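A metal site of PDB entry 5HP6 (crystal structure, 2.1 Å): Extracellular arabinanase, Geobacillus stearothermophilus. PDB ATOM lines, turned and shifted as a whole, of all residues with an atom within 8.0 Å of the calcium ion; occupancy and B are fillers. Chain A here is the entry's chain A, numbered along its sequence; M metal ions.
Of the 21 residues printed, 6 come within 4 Å of the calcium ion.
The nearest printed residue that does not touch the calcium ion is Gly 687 (4.2 Å).
The calcium ion is bound by O of Ile 686, O of Ser 649, O of Lys 688, OD1 of Asp 826, OE2 of Glu 827 and OD1 of Asp 651.
Slightly farther from the calcium ion lies OD2 of Asp 826 (3.1 Å).
OD2 of Asp 826 sits at hydrogen-bond distance from N of Lys 685.
A ring nitrogen (NE2) of His 647 lies within hydrogen-bond range of the side-chain carboxylate of Glu 827 (3.2 Å).
The backbone NH (N) of Asp 826 is in hydrogen-bond range of the backbone carbonyl oxygen (O) of Trp 715 (2.8 Å).
The side-chain amino group of Lys 688 is in salt-bridge range of the side-chain carboxylate of Asp 683, at 3.3 Å.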
ATOM      1  N   HIS A 647       7.265  15.206  -9.590  1.00  0.00           N
ATOM      2  CA  HIS A 647       6.394  14.042  -9.478  1.00  0.00           C
ATOM      3  C   HIS A 647       4.948  14.500  -9.575  1.00  0.00           C
ATOM      4  O   HIS A 647       4.393  15.007  -8.623  1.00  0.00           O
ATOM      5  CB  HIS A 647       6.649  13.306  -8.153  1.00  0.00           C
ATOM      6  CG  HIS A 647       5.683  12.182  -7.876  1.00  0.00           C
ATOM      7  ND1 HIS A 647       5.431  11.722  -6.601  1.00  0.00           N
ATOM      8  CD2 HIS A 647       4.923  11.442  -8.709  1.00  0.00           C
ATOM      9  CE1 HIS A 647       4.551  10.736  -6.658  1.00  0.00           C
ATOM     10  NE2 HIS A 647       4.221  10.549  -7.921  1.00  0.00           N
ATOM     11  N   TYR A 648       4.356  14.341 -10.759  1.00  0.00           N
ATOM     12  CA  TYR A 648       2.939  14.666 -10.938  1.00  0.00           C
ATOM     13  C   TYR A 648       2.110  13.399 -10.771  1.00  0.00           C
ATOM     14  O   TYR A 648       2.076  12.549 -11.668  1.00  0.00           O
ATOM     15  CB  TYR A 648       2.716  15.298 -12.315  1.00  0.00           C
ATOM     16  CG  TYR A 648       3.386  16.648 -12.457  1.00  0.00           C
ATOM     17  CD1 TYR A 648       4.700  16.740 -12.908  1.00  0.00           C
ATOM     18  CD2 TYR A 648       2.719  17.824 -12.115  1.00  0.00           C
ATOM     19  CE1 TYR A 648       5.329  17.960 -13.023  1.00  0.00           C
ATOM     20  CE2 TYR A 648       3.344  19.036 -12.224  1.00  0.00           C
ATOM     21  CZ  TYR A 648       4.646  19.102 -12.684  1.00  0.00           C
ATOM     22  OH  TYR A 648       5.266  20.324 -12.803  1.00  0.00           O
ATOM     23  N   SER A 649       1.463  13.264  -9.621  1.00  0.00           N
ATOM     24  CA  SER A 649       0.751  12.030  -9.296  1.00  0.00           C
ATOM     25  C   SER A 649      -0.739  12.102  -9.618  1.00  0.00           C
ATOM     26  O   SER A 649      -1.386  11.074  -9.777  1.00  0.00           O
ATOM     27  CB  SER A 649       0.935  11.681  -7.814  1.00  0.00           C
ATOM     28  OG  SER A 649       0.229  12.591  -6.999  1.00  0.00           O
ATOM     29  N   PHE A 650      -1.276  13.312  -9.712  1.00  0.00           N
ATOM     30  CA  PHE A 650      -2.713  13.559  -9.886  1.00  0.00           C
ATOM     31  C   PHE A 650      -3.545  12.979  -8.743  1.00  0.00           C
ATOM     32  O   PHE A 650      -4.768  12.875  -8.871  1.00  0.00           O
ATOM     33  CB  PHE A 650      -3.225  12.980 -11.211  1.00  0.00           C
ATOM     34  CG  PHE A 650      -2.350  13.278 -12.394  1.00  0.00           C
ATOM     35  CD1 PHE A 650      -2.381  14.516 -13.004  1.00  0.00           C
ATOM     36  CD2 PHE A 650      -1.508  12.300 -12.913  1.00  0.00           C
ATOM     37  CE1 PHE A 650      -1.579  14.787 -14.106  1.00  0.00           C
ATOM     38  CE2 PHE A 650      -0.702  12.562 -14.006  1.00  0.00           C
ATOM     39  CZ  PHE A 650      -0.736  13.812 -14.601  1.00  0.00           C
ATOM     40  N   ASP A 651      -2.887  12.622  -7.641  1.00  0.00           N
ATOM     41  CA  ASP A 651      -3.535  11.939  -6.512  1.00  0.00           C
ATOM     42  C   ASP A 651      -4.547  12.820  -5.778  1.00  0.00           C
ATOM     43  O   ASP A 651      -5.365  12.323  -5.009  1.00  0.00           O
ATOM     44  CB  ASP A 651      -2.490  11.438  -5.509  1.00  0.00           C
ATOM     45  CG  ASP A 651      -1.733  10.221  -6.003  1.00  0.00           C
ATOM     46  OD1 ASP A 651      -2.188   9.599  -6.994  1.00  0.00           O
ATOM     47  OD2 ASP A 651      -0.697   9.867  -5.392  1.00  0.00           O
ATOM     48  N   ASN A 652      -4.458  14.130  -6.011  1.00  0.00           N
ATOM     49  CA  ASN A 652      -5.350  15.087  -5.385  1.00  0.00           C
ATOM     50  C   ASN A 652      -6.279  15.742  -6.402  1.00  0.00           C
ATOM     51  O   ASN A 652      -6.728  16.870  -6.201  1.00  0.00           O
ATOM     52  CB  ASN A 652      -4.544  16.157  -4.646  1.00  0.00           C
ATOM     53  CG  ASN A 652      -3.610  15.563  -3.611  1.00  0.00           C
ATOM     54  OD1 ASN A 652      -3.953  14.589  -2.927  1.00  0.00           O
ATOM     55  ND2 ASN A 652      -2.414  16.130  -3.493  1.00  0.00           N
ATOM     56  N   ALA A 682      -9.814   9.839 -12.967  1.00  0.00           N
ATOM     57  CA  ALA A 682     -10.351   8.505 -12.660  1.00  0.00           C
ATOM     58  C   ALA A 682      -9.387   7.681 -11.812  1.00  0.00           C
ATOM     59  O   ALA A 682      -8.293   8.147 -11.510  1.00  0.00           O
ATOM     60  CB  ALA A 682     -10.689   7.765 -13.956  1.00  0.00           C
ATOM     61  N   ASP A 683      -9.774   6.458 -11.438  1.00  0.00           N
ATOM     62  CA  ASP A 683      -8.894   5.584 -10.651  1.00  0.00           C
ATOM     63  C   ASP A 683      -7.745   5.066 -11.519  1.00  0.00           C
ATOM     64  O   ASP A 683      -7.967   4.516 -12.598  1.00  0.00           O
ATOM     65  CB  ASP A 683      -9.668   4.409 -10.049  1.00  0.00           C
ATOM     66  CG  ASP A 683     -10.901   4.849  -9.283  1.00  0.00           C
ATOM     67  OD1 ASP A 683     -11.012   6.045  -8.957  1.00  0.00           O
ATOM     68  OD2 ASP A 683     -11.752   3.975  -8.992  1.00  0.00           O
ATOM     69  N   GLY A 684      -6.516   5.233 -11.037  1.00  0.00           N
ATOM     70  CA  GLY A 684      -5.346   4.926 -11.846  1.00  0.00           C
ATOM     71  C   GLY A 684      -4.586   3.713 -11.368  1.00  0.00           C
ATOM     72  O   GLY A 684      -5.149   2.849 -10.685  1.00  0.00           O
ATOM     73  N   LYS A 685      -3.309   3.642 -11.738  1.00  0.00           N
ATOM     74  CA  LYS A 685      -2.418   2.560 -11.316  1.00  0.00           C
ATOM     75  C   LYS A 685      -2.020   2.775  -9.862  1.00  0.00           C
ATOM     76  O   LYS A 685      -2.019   1.838  -9.055  1.00  0.00           O
ATOM     77  CB  LYS A 685      -1.173   2.501 -12.225  1.00  0.00           C
ATOM     78  CG  LYS A 685      -0.447   1.158 -12.224  1.00  0.00           C
ATOM     79  CD  LYS A 685      -1.350   0.026 -12.718  1.00  0.00           C
ATOM     80  CE  LYS A 685      -0.607  -1.314 -12.858  1.00  0.00           C
ATOM     81  NZ  LYS A 685      -0.707  -2.222 -11.671  1.00  0.00           N
ATOM     82  N   ILE A 686      -1.677   4.016  -9.534  1.00  0.00           N
ATOM     83  CA  ILE A 686      -1.465   4.408  -8.150  1.00  0.00           C
ATOM     84  C   ILE A 686      -2.366   5.595  -7.851  1.00  0.00           C
ATOM     85  O   ILE A 686      -2.030   6.738  -8.149  1.00  0.00           O
ATOM     86  CB  ILE A 686      -0.002   4.792  -7.870  1.00  0.00           C
ATOM     87  CG1 ILE A 686       0.926   3.590  -8.111  1.00  0.00           C
ATOM     88  CG2 ILE A 686       0.132   5.317  -6.443  1.00  0.00           C
ATOM     89  CD1 ILE A 686       2.322   3.731  -7.540  1.00  0.00           C
ATOM     90  N   GLY A 687      -3.533   5.301  -7.280  1.00  0.00           N
ATOM     91  CA  GLY A 687      -4.482   6.322  -6.875  1.00  0.00           C
ATOM     92  C   GLY A 687      -5.328   6.851  -8.019  1.00  0.00           C
ATOM     93  O   GLY A 687      -5.787   6.092  -8.888  1.00  0.00           O
ATOM     94  N   LYS A 688      -5.537   8.169  -7.996  1.00  0.00           N
ATOM     95  CA  LYS A 688      -6.210   8.882  -9.085  1.00  0.00           C
ATOM     96  C   LYS A 688      -5.228   9.134 -10.255  1.00  0.00           C
ATOM     97  O   LYS A 688      -4.025   9.318 -10.040  1.00  0.00           O
ATOM     98  CB  LYS A 688      -6.767  10.217  -8.555  1.00  0.00           C
ATOM     99  CG  LYS A 688      -8.193  10.573  -9.008  1.00  0.00           C
ATOM    100  CD  LYS A 688      -9.225   9.500  -8.683  1.00  0.00           C
ATOM    101  CE  LYS A 688     -10.640  10.049  -8.935  1.00  0.00           C
ATOM    102  NZ  LYS A 688     -11.736   9.177  -8.435  1.00  0.00           N
ATOM    103  N   ALA A 689      -5.723   9.115 -11.487  1.00  0.00           N
ATOM    104  CA  ALA A 689      -4.899   9.461 -12.655  1.00  0.00           C
ATOM    105  C   ALA A 689      -5.573  10.565 -13.467  1.00  0.00           C
ATOM    106  O   ALA A 689      -6.702  10.970 -13.167  1.00  0.00           O
ATOM    107  CB  ALA A 689      -4.641   8.238 -13.519  1.00  0.00           C
ATOM    108  N   ALA A 690      -4.875  11.069 -14.494  1.00  0.00           N
ATOM    109  CA  ALA A 690      -5.402  12.135 -15.330  1.00  0.00           C
ATOM    110  C   ALA A 690      -6.005  11.593 -16.630  1.00  0.00           C
ATOM    111  O   ALA A 690      -5.438  10.716 -17.286  1.00  0.00           O
ATOM    112  CB  ALA A 690      -4.312  13.164 -15.657  1.00  0.00           C
ATOM    113  N   TRP A 715       3.067   5.945 -16.230  1.00  0.00           N
ATOM    114  CA  TRP A 715       2.112   4.900 -16.611  1.00  0.00           C
ATOM    115  C   TRP A 715       1.131   5.470 -17.600  1.00  0.00           C
ATOM    116  O   TRP A 715       0.631   6.586 -17.416  1.00  0.00           O
ATOM    117  CB  TRP A 715       1.352   4.372 -15.374  1.00  0.00           C
ATOM    118  CG  TRP A 715       2.207   3.623 -14.417  1.00  0.00           C
ATOM    119  CD1 TRP A 715       2.900   4.141 -13.362  1.00  0.00           C
ATOM    120  CD2 TRP A 715       2.447   2.208 -14.406  1.00  0.00           C
ATOM    121  NE1 TRP A 715       3.571   3.131 -12.703  1.00  0.00           N
ATOM    122  CE2 TRP A 715       3.316   1.943 -13.336  1.00  0.00           C
ATOM    123  CE3 TRP A 715       2.023   1.150 -15.226  1.00  0.00           C
ATOM    124  CZ2 TRP A 715       3.750   0.658 -13.040  1.00  0.00           C
ATOM    125  CZ3 TRP A 715       2.474  -0.122 -14.936  1.00  0.00           C
ATOM    126  CH2 TRP A 715       3.328  -0.366 -13.847  1.00  0.00           C
ATOM    127  N   TRP A 772      -2.577  -1.055 -18.669  1.00  0.00           N
ATOM    128  CA  TRP A 772      -1.542  -0.187 -18.102  1.00  0.00           C
ATOM    129  C   TRP A 772      -0.152  -0.600 -18.549  1.00  0.00           C
ATOM    130  O   TRP A 772       0.297  -1.716 -18.279  1.00  0.00           O
ATOM    131  CB  TRP A 772      -1.613  -0.196 -16.577  1.00  0.00           C
ATOM    132  CG  TRP A 772      -2.768   0.597 -16.044  1.00  0.00           C
ATOM    133  CD1 TRP A 772      -3.940   0.110 -15.531  1.00  0.00           C
ATOM    134  CD2 TRP A 772      -2.859   2.027 -15.978  1.00  0.00           C
ATOM    135  NE1 TRP A 772      -4.754   1.153 -15.147  1.00  0.00           N
ATOM    136  CE2 TRP A 772      -4.116   2.340 -15.403  1.00  0.00           C
ATOM    137  CE3 TRP A 772      -2.006   3.074 -16.340  1.00  0.00           C
ATOM    138  CZ2 TRP A 772      -4.538   3.653 -15.197  1.00  0.00           C
ATOM    139  CZ3 TRP A 772      -2.423   4.377 -16.125  1.00  0.00           C
ATOM    140  CH2 TRP A 772      -3.674   4.660 -15.552  1.00  0.00           C
ATOM    141  N   ILE A 825      -3.155   8.819 -18.113  1.00  0.00           N
ATOM    142  CA  ILE A 825      -1.765   9.036 -17.746  1.00  0.00           C
ATOM    143  C   ILE A 825      -1.628   9.081 -16.237  1.00  0.00           C
ATOM    144  O   ILE A 825      -2.425   9.741 -15.572  1.00  0.00           O
ATOM    145  CB  ILE A 825      -1.210  10.365 -18.303  1.00  0.00           C
ATOM    146  CG1 ILE A 825      -1.516  10.493 -19.798  1.00  0.00           C
ATOM    147  CG2 ILE A 825       0.289  10.490 -18.031  1.00  0.00           C
ATOM    148  CD1 ILE A 825      -0.789   9.494 -20.654  1.00  0.00           C
ATOM    149  N   ASP A 826      -0.638   8.397 -15.688  1.00  0.00           N
ATOM    150  CA  ASP A 826      -0.435   8.422 -14.238  1.00  0.00           C
ATOM    151  C   ASP A 826       1.027   8.436 -13.808  1.00  0.00           C
ATOM    152  O   ASP A 826       1.903   7.982 -14.551  1.00  0.00           O
ATOM    153  CB  ASP A 826      -1.141   7.223 -13.600  1.00  0.00           C
ATOM    154  CG  ASP A 826      -1.370   7.424 -12.114  1.00  0.00           C
ATOM    155  OD1 ASP A 826      -1.684   8.565 -11.731  1.00  0.00           O
ATOM    156  OD2 ASP A 826      -1.252   6.442 -11.344  1.00  0.00           O
ATOM    157  N   GLU A 827       1.277   8.982 -12.615  1.00  0.00           N
ATOM    158  CA  GLU A 827       2.591   8.990 -11.972  1.00  0.00           C
ATOM    159  C   GLU A 827       3.735   9.478 -12.858  1.00  0.00           C
ATOM    160  O   GLU A 827       4.705   8.747 -13.084  1.00  0.00           O
ATOM    161  CB  GLU A 827       2.925   7.590 -11.454  1.00  0.00           C
ATOM    162  CG  GLU A 827       1.861   6.993 -10.552  1.00  0.00           C
ATOM    163  CD  GLU A 827       1.670   7.798  -9.287  1.00  0.00           C
ATOM    164  OE1 GLU A 827       2.576   7.793  -8.426  1.00  0.00           O
ATOM    165  OE2 GLU A 827       0.588   8.414  -9.142  1.00  0.00           O
ATOM    166  N   LEU A 828       3.629  10.696 -13.381  1.00  0.00           N
ATOM    167  CA  LEU A 828       4.734  11.266 -14.134  1.00  0.00           C
ATOM    168  C   LEU A 828       5.882  11.605 -13.197  1.00  0.00           C
ATOM    169  O   LEU A 828       5.762  12.466 -12.322  1.00  0.00           O
ATOM    170  CB  LEU A 828       4.297  12.511 -14.906  1.00  0.00           C
ATOM    171  CG  LEU A 828       5.423  13.272 -15.610  1.00  0.00           C
ATOM    172  CD1 LEU A 828       6.065  12.431 -16.705  1.00  0.00           C
ATOM    173  CD2 LEU A 828       4.877  14.580 -16.174  1.00  0.00           C
HETATM  174 CA    CA M   1      -1.799   8.772  -9.323  1.00  0.00          CA
